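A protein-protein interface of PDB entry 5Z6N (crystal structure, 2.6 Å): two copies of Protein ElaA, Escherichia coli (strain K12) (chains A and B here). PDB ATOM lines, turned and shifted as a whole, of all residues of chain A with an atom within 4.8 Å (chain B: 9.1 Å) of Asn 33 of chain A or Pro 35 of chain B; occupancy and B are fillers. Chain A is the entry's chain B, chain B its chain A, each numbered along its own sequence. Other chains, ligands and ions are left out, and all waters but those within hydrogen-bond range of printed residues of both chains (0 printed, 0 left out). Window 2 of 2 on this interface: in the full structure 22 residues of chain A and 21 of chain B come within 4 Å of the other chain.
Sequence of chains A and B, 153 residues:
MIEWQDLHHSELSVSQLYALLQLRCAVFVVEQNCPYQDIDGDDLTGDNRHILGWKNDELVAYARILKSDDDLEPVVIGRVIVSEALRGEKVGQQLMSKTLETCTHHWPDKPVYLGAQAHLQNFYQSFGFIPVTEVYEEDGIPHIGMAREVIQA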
ATOM      1  N   VAL A  29     -11.817 -28.916  15.330  1.00  0.00           N
ATOM      2  CA  VAL A  29     -13.165 -28.729  15.850  1.00  0.00           C
ATOM      3  C   VAL A  29     -13.249 -27.506  16.752  1.00  0.00           C
ATOM      4  O   VAL A  29     -14.040 -26.595  16.505  1.00  0.00           O
ATOM      5  CB  VAL A  29     -13.646 -30.000  16.583  1.00  0.00           C
ATOM      6  CG1 VAL A  29     -14.981 -29.742  17.262  1.00  0.00           C
ATOM      7  CG2 VAL A  29     -13.764 -31.161  15.609  1.00  0.00           C
ATOM      8  N   VAL A  30     -12.421 -27.466  17.798  1.00  0.00           N
ATOM      9  CA  VAL A  30     -12.524 -26.458  18.847  1.00  0.00           C
ATOM     10  C   VAL A  30     -11.965 -25.090  18.479  1.00  0.00           C
ATOM     11  O   VAL A  30     -12.664 -24.073  18.561  1.00  0.00           O
ATOM     12  CB  VAL A  30     -11.796 -26.936  20.114  1.00  0.00           C
ATOM     13  CG1 VAL A  30     -11.932 -25.913  21.219  1.00  0.00           C
ATOM     14  CG2 VAL A  30     -12.354 -28.273  20.565  1.00  0.00           C
ATOM     15  N   GLU A  31     -10.693 -25.061  18.072  1.00  0.00           N
ATOM     16  CA  GLU A  31      -9.997 -23.794  17.879  1.00  0.00           C
ATOM     17  C   GLU A  31     -10.403 -23.217  16.528  1.00  0.00           C
ATOM     18  O   GLU A  31     -10.492 -21.993  16.368  1.00  0.00           O
ATOM     19  CB  GLU A  31      -8.482 -23.990  17.966  1.00  0.00           C
ATOM     20  CG  GLU A  31      -7.645 -23.188  16.977  1.00  0.00           C
ATOM     21  CD  GLU A  31      -6.186 -23.601  17.000  1.00  0.00           C
ATOM     22  OE1 GLU A  31      -5.322 -22.743  16.729  1.00  0.00           O
ATOM     23  OE2 GLU A  31      -5.914 -24.783  17.292  1.00  0.00           O
ATOM     24  N   GLN A  32     -10.646 -24.074  15.543  1.00  0.00           N
ATOM     25  CA  GLN A  32     -11.064 -23.621  14.226  1.00  0.00           C
ATOM     26  C   GLN A  32     -12.575 -23.461  14.110  1.00  0.00           C
ATOM     27  O   GLN A  32     -13.072 -23.193  13.010  1.00  0.00           O
ATOM     28  CB  GLN A  32     -10.535 -24.568  13.142  1.00  0.00           C
ATOM     29  CG  GLN A  32      -9.194 -24.105  12.577  1.00  0.00           C
ATOM     30  CD  GLN A  32      -8.478 -25.157  11.753  1.00  0.00           C
ATOM     31  OE1 GLN A  32      -9.105 -26.024  11.142  1.00  0.00           O
ATOM     32  NE2 GLN A  32      -7.152 -25.080  11.727  1.00  0.00           N
ATOM     33  N   ASN A  33     -13.310 -23.615  15.217  1.00  0.00           N
ATOM     34  CA  ASN A  33     -14.723 -23.235  15.294  1.00  0.00           C
ATOM     35  C   ASN A  33     -15.543 -23.907  14.189  1.00  0.00           C
ATOM     36  O   ASN A  33     -16.258 -23.254  13.427  1.00  0.00           O
ATOM     37  CB  ASN A  33     -14.862 -21.710  15.238  1.00  0.00           C
ATOM     38  CG  ASN A  33     -16.260 -21.230  15.564  1.00  0.00           C
ATOM     39  OD1 ASN A  33     -16.861 -21.646  16.554  1.00  0.00           O
ATOM     40  ND2 ASN A  33     -16.790 -20.349  14.724  1.00  0.00           N
ATOM     41  N   CYS A  34     -15.429 -25.233  14.101  1.00  0.00           N
ATOM     42  CA  CYS A  34     -16.014 -25.986  12.993  1.00  0.00           C
ATOM     43  C   CYS A  34     -16.637 -27.280  13.502  1.00  0.00           C
ATOM     44  O   CYS A  34     -15.981 -28.329  13.545  1.00  0.00           O
ATOM     45  CB  CYS A  34     -14.966 -26.275  11.918  1.00  0.00           C
ATOM     46  SG  CYS A  34     -15.572 -27.218  10.502  1.00  0.00           S
ATOM     47  N   PRO A  35     -17.920 -27.245  13.890  1.00  0.00           N
ATOM     48  CA  PRO A  35     -18.583 -28.474  14.350  1.00  0.00           C
ATOM     49  C   PRO A  35     -18.673 -29.329  13.095  1.00  0.00           C
ATOM     50  O   PRO A  35     -19.380 -28.974  12.146  1.00  0.00           O
ATOM     51  CB  PRO A  35     -19.907 -27.963  14.935  1.00  0.00           C
ATOM     52  CG  PRO A  35     -20.146 -26.652  14.254  1.00  0.00           C
ATOM     53  CD  PRO A  35     -18.789 -26.060  14.012  1.00  0.00           C
ATOM     54  N   ASP A 139     -14.614 -22.796   5.010  1.00  0.00           N
ATOM     55  CA  ASP A 139     -14.843 -21.777   6.030  1.00  0.00           C
ATOM     56  C   ASP A 139     -14.192 -20.541   5.420  1.00  0.00           C
ATOM     57  O   ASP A 139     -13.321 -20.666   4.553  1.00  0.00           O
ATOM     58  CB  ASP A 139     -14.375 -22.294   7.391  1.00  0.00           C
ATOM     59  CG  ASP A 139     -14.955 -21.495   8.547  1.00  0.00           C
ATOM     60  OD1 ASP A 139     -14.460 -20.379   8.813  1.00  0.00           O
ATOM     61  OD2 ASP A 139     -15.916 -21.979   9.182  1.00  0.00           O
ATOM     62  N   CYS B  25     -18.806 -37.493  19.087  1.00  0.00           N
ATOM     63  CA  CYS B  25     -18.657 -36.409  18.122  1.00  0.00           C
ATOM     64  C   CYS B  25     -19.929 -36.246  17.298  1.00  0.00           C
ATOM     65  O   CYS B  25     -20.391 -35.124  17.056  1.00  0.00           O
ATOM     66  CB  CYS B  25     -17.454 -36.675  17.215  1.00  0.00           C
ATOM     67  SG  CYS B  25     -17.091 -35.354  16.030  1.00  0.00           S
ATOM     68  N   PHE B  28     -22.828 -34.827  20.183  1.00  0.00           N
ATOM     69  CA  PHE B  28     -22.695 -33.601  20.958  1.00  0.00           C
ATOM     70  C   PHE B  28     -22.043 -32.457  20.190  1.00  0.00           C
ATOM     71  O   PHE B  28     -22.184 -31.299  20.605  1.00  0.00           O
ATOM     72  CB  PHE B  28     -21.921 -33.885  22.250  1.00  0.00           C
ATOM     73  CG  PHE B  28     -22.639 -34.827  23.174  1.00  0.00           C
ATOM     74  CD1 PHE B  28     -23.855 -34.466  23.734  1.00  0.00           C
ATOM     75  CD2 PHE B  28     -22.114 -36.074  23.472  1.00  0.00           C
ATOM     76  CE1 PHE B  28     -24.533 -35.325  24.575  1.00  0.00           C
ATOM     77  CE2 PHE B  28     -22.787 -36.940  24.319  1.00  0.00           C
ATOM     78  CZ  PHE B  28     -23.999 -36.565  24.869  1.00  0.00           C
ATOM     79  N   VAL B  29     -21.350 -32.740  19.084  1.00  0.00           N
ATOM     80  CA  VAL B  29     -20.628 -31.692  18.363  1.00  0.00           C
ATOM     81  C   VAL B  29     -21.156 -31.376  16.969  1.00  0.00           C
ATOM     82  O   VAL B  29     -21.155 -30.213  16.555  1.00  0.00           O
ATOM     83  CB  VAL B  29     -19.148 -32.053  18.157  1.00  0.00           C
ATOM     84  CG1 VAL B  29     -18.516 -31.095  17.150  1.00  0.00           C
ATOM     85  CG2 VAL B  29     -18.413 -32.014  19.479  1.00  0.00           C
ATOM     86  N   VAL B  30     -21.607 -32.381  16.220  1.00  0.00           N
ATOM     87  CA  VAL B  30     -22.054 -32.081  14.863  1.00  0.00           C
ATOM     88  C   VAL B  30     -23.562 -31.859  14.969  1.00  0.00           C
ATOM     89  O   VAL B  30     -24.069 -30.827  14.521  1.00  0.00           O
ATOM     90  CB  VAL B  30     -21.669 -33.141  13.806  1.00  0.00           C
ATOM     91  CG1 VAL B  30     -22.258 -34.497  14.088  1.00  0.00           C
ATOM     92  CG2 VAL B  30     -22.061 -32.656  12.403  1.00  0.00           C
ATOM     93  N   GLU B  31     -24.288 -32.776  15.625  1.00  0.00           N
ATOM     94  CA  GLU B  31     -25.750 -32.685  15.666  1.00  0.00           C
ATOM     95  C   GLU B  31     -26.208 -31.470  16.469  1.00  0.00           C
ATOM     96  O   GLU B  31     -26.959 -30.625  15.969  1.00  0.00           O
ATOM     97  CB  GLU B  31     -26.333 -33.978  16.236  1.00  0.00           C
ATOM     98  CG  GLU B  31     -27.820 -34.164  15.996  1.00  0.00           C
ATOM     99  CD  GLU B  31     -28.398 -35.187  16.945  1.00  0.00           C
ATOM    100  OE1 GLU B  31     -29.600 -35.100  17.289  1.00  0.00           O
ATOM    101  OE2 GLU B  31     -27.630 -36.080  17.355  1.00  0.00           O
ATOM    102  N   GLN B  32     -25.754 -31.360  17.722  1.00  0.00           N
ATOM    103  CA  GLN B  32     -26.057 -30.231  18.598  1.00  0.00           C
ATOM    104  C   GLN B  32     -25.287 -28.954  18.268  1.00  0.00           C
ATOM    105  O   GLN B  32     -25.366 -27.987  19.040  1.00  0.00           O
ATOM    106  CB  GLN B  32     -25.908 -30.657  20.062  1.00  0.00           C
ATOM    107  CG  GLN B  32     -26.802 -31.828  20.445  1.00  0.00           C
ATOM    108  CD  GLN B  32     -26.537 -32.372  21.843  1.00  0.00           C
ATOM    109  OE1 GLN B  32     -27.196 -33.308  22.281  1.00  0.00           O
ATOM    110  NE2 GLN B  32     -25.574 -31.791  22.543  1.00  0.00           N
ATOM    111  N   ASN B  33     -24.564 -28.957  17.142  1.00  0.00           N
ATOM    112  CA  ASN B  33     -23.869 -27.801  16.580  1.00  0.00           C
ATOM    113  C   ASN B  33     -22.890 -27.084  17.499  1.00  0.00           C
ATOM    114  O   ASN B  33     -22.690 -25.870  17.386  1.00  0.00           O
ATOM    115  CB  ASN B  33     -24.816 -26.828  15.870  1.00  0.00           C
ATOM    116  CG  ASN B  33     -24.076 -25.747  15.102  1.00  0.00           C
ATOM    117  OD1 ASN B  33     -24.008 -24.600  15.541  1.00  0.00           O
ATOM    118  ND2 ASN B  33     -23.512 -26.109  13.954  1.00  0.00           N
ATOM    119  N   CYS B  34     -22.297 -27.825  18.431  1.00  0.00           N
ATOM    120  CA  CYS B  34     -21.394 -27.253  19.425  1.00  0.00           C
ATOM    121  C   CYS B  34     -19.926 -27.619  19.249  1.00  0.00           C
ATOM    122  O   CYS B  34     -19.564 -28.802  19.403  1.00  0.00           O
ATOM    123  CB  CYS B  34     -21.930 -27.774  20.754  1.00  0.00           C
ATOM    124  SG  CYS B  34     -21.047 -27.143  22.193  1.00  0.00           S
ATOM    125  N   PRO B  35     -19.084 -26.687  18.952  1.00  0.00           N
ATOM    126  CA  PRO B  35     -17.660 -26.983  18.712  1.00  0.00           C
ATOM    127  C   PRO B  35     -16.848 -26.943  20.006  1.00  0.00           C
ATOM    128  O   PRO B  35     -16.110 -26.003  20.308  1.00  0.00           O
ATOM    129  CB  PRO B  35     -17.250 -25.875  17.741  1.00  0.00           C
ATOM    130  CG  PRO B  35     -18.205 -24.714  18.051  1.00  0.00           C
ATOM    131  CD  PRO B  35     -19.339 -25.238  18.911  1.00  0.00           C
ATOM    132  N   TYR B  36     -16.994 -27.992  20.804  1.00  0.00           N
ATOM    133  CA  TYR B  36     -16.332 -28.087  22.097  1.00  0.00           C
ATOM    134  C   TYR B  36     -15.393 -29.289  22.101  1.00  0.00           C
ATOM    135  O   TYR B  36     -15.336 -30.069  21.146  1.00  0.00           O
ATOM    136  CB  TYR B  36     -17.360 -28.169  23.234  1.00  0.00           C
ATOM    137  CG  TYR B  36     -17.879 -29.562  23.517  1.00  0.00           C
ATOM    138  CD1 TYR B  36     -18.737 -30.200  22.630  1.00  0.00           C
ATOM    139  CD2 TYR B  36     -17.517 -30.234  24.678  1.00  0.00           C
ATOM    140  CE1 TYR B  36     -19.212 -31.470  22.889  1.00  0.00           C
ATOM    141  CE2 TYR B  36     -17.989 -31.506  24.944  1.00  0.00           C
ATOM    142  CZ  TYR B  36     -18.834 -32.120  24.046  1.00  0.00           C
ATOM    143  OH  TYR B  36     -19.304 -33.387  24.309  1.00  0.00           O
ATOM    144  N   GLN B  37     -14.644 -29.422  23.194  1.00  0.00           N
ATOM    145  CA  GLN B  37     -13.641 -30.473  23.353  1.00  0.00           C
ATOM    146  C   GLN B  37     -14.305 -31.672  24.022  1.00  0.00           C
ATOM    147  O   GLN B  37     -14.294 -31.815  25.244  1.00  0.00           O
ATOM    148  CB  GLN B  37     -12.456 -29.954  24.162  1.00  0.00           C
ATOM    149  CG  GLN B  37     -11.372 -30.980  24.446  1.00  0.00           C
ATOM    150  CD  GLN B  37     -10.834 -31.620  23.186  1.00  0.00           C
ATOM    151  OE1 GLN B  37     -11.265 -32.703  22.793  1.00  0.00           O
ATOM    152  NE2 GLN B  37      -9.889 -30.949  22.540  1.00  0.00           N
ATOM    153  N   ASP B  38     -14.901 -32.546  23.205  1.00  0.00           N
ATOM    154  CA  ASP B  38     -15.532 -33.749  23.743  1.00  0.00           C
ATOM    155  C   ASP B  38     -14.494 -34.707  24.308  1.00  0.00           C
ATOM    156  O   ASP B  38     -14.696 -35.296  25.378  1.00  0.00           O
ATOM    157  CB  ASP B  38     -16.363 -34.440  22.660  1.00  0.00           C
ATOM    158  CG  ASP B  38     -16.820 -35.829  23.073  1.00  0.00           C
ATOM    159  OD1 ASP B  38     -17.764 -35.934  23.884  1.00  0.00           O
ATOM    160  OD2 ASP B  38     -16.232 -36.819  22.589  1.00  0.00           O
ATOM    161  N   ASP B 139     -22.622 -25.397  26.941  1.00  0.00           N
ATOM    162  CA  ASP B 139     -22.538 -25.848  25.578  1.00  0.00           C
ATOM    163  C   ASP B 139     -22.429 -27.354  25.495  1.00  0.00           C
ATOM    164  O   ASP B 139     -22.024 -28.000  26.429  1.00  0.00           O
ATOM    165  CB  ASP B 139     -21.376 -25.145  24.880  1.00  0.00           C
ATOM    166  CG  ASP B 139     -19.997 -25.702  25.273  1.00  0.00           C
ATOM    167  OD1 ASP B 139     -19.903 -26.623  26.121  1.00  0.00           O
ATOM    168  OD2 ASP B 139     -19.004 -25.213  24.689  1.00  0.00           O
ATOM    169  N   ILE B 141     -29.315 -23.929  25.133  1.00  0.00           N
ATOM    170  CA  ILE B 141     -28.503 -24.737  26.034  1.00  0.00           C
ATOM    171  C   ILE B 141     -28.788 -24.474  27.524  1.00  0.00           C
ATOM    172  O   ILE B 141     -27.858 -24.219  28.284  1.00  0.00           O
ATOM    173  CB  ILE B 141     -27.004 -24.500  25.740  1.00  0.00           C
ATOM    174  CG1 ILE B 141     -26.794 -24.247  24.245  1.00  0.00           C
ATOM    175  CG2 ILE B 141     -26.160 -25.679  26.213  1.00  0.00           C
ATOM    176  CD1 ILE B 141     -25.369 -23.891  23.876  1.00  0.00           C
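Pro 35 of chain B touches three residues of chain A.
Of chain B, only Pro 35, Tyr 36 and Gln 37 come within 4 Å of Val 30 of chain A.
Cys 34 of chain A touches none of the printed residues of chain B.
Of the printed residues of chain B, Pro 35 of chain A touches Val 29 (3.0 Å) and Asn 33 (3.4 Å).
Of the printed residues of chain A, Val 29 of chain B touches Val 29 (3.8 Å) and Pro 35 (3.0 Å).
Printed residues of chain B within 4 Å of Val 29 of chain A: Val 29, Pro 35 and Tyr 36.
Ile 141 of chain B touches none of the printed residues of chain A.
Phe 28 of chain B touches none of the printed residues of chain A.
Val 29 of chain A touches its own counterpart, Val 29 of chain B.
Val 29 of chain A touches Pro 35 of chain B, and with the chains exchanged Pro 35 of chain A touches Val 29 of chain B.
Val 30 of chain A touches Pro 35 of chain B, but with the chains exchanged Pro 35 of chain A does not touch Val 30 of chain B (4.6 Å).
Asn 33 of chain A touches Pro 35 of chain B, and with the chains exchanged Pro 35 of chain A touches Asn 33 of chain B.
Among the printed residues, pairs that only touch across the chains: Pro 35 of chain A with Val 29 of chain B (3.0 Å), Pro 35 of chain A with Asn 33 of chain B (3.4 Å), Val 29 of chain A with Pro 35 of chain B (3.5 Å), Val 30 of chain A with Tyr 36 of chain B (3.5 Å), Asn 33 of chain A with Pro 35 of chain B (3.7 Å), Val 30 of chain A with Gln 37 of chain B (3.7 Å), Val 29 of chain A with Val 29 of chain B (3.8 Å), Val 30 of chain A with Pro 35 of chain B (3.9 Å) and Val 29 of chain A with Tyr 36 of chain B (3.9 Å).
N of Cys 34 of chain B lies within hydrogen-bond range of O of Val 29 of chain B.
The side-chain hydroxyl (OH) of Tyr 36 of chain B lies within hydrogen-bond range of the side-chain carboxylate (OD1) of Asp 38 of chain B (3.0 Å).
The backbone carbonyl oxygen (O) of Val 29 of chain A is in hydrogen-bond range of the backbone NH (N) of Cys 34 of chain A.
Of the 14 printed residues of chain B, 5 touch a printed residue of chain A.
Hydrophobic or aromatic side chains of chain B that line the printed part of chain A: Val 29 and Pro 35.
Along chain B the printed residues that touch a printed residue of chain A span positions 29 to 37.
Among the printed residues, 9 pairs touch across the chains.
Among the printed residues, no Asp or Glu carboxylate lies within 4 Å of a Lys or Arg side-chain nitrogen of the other chain.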
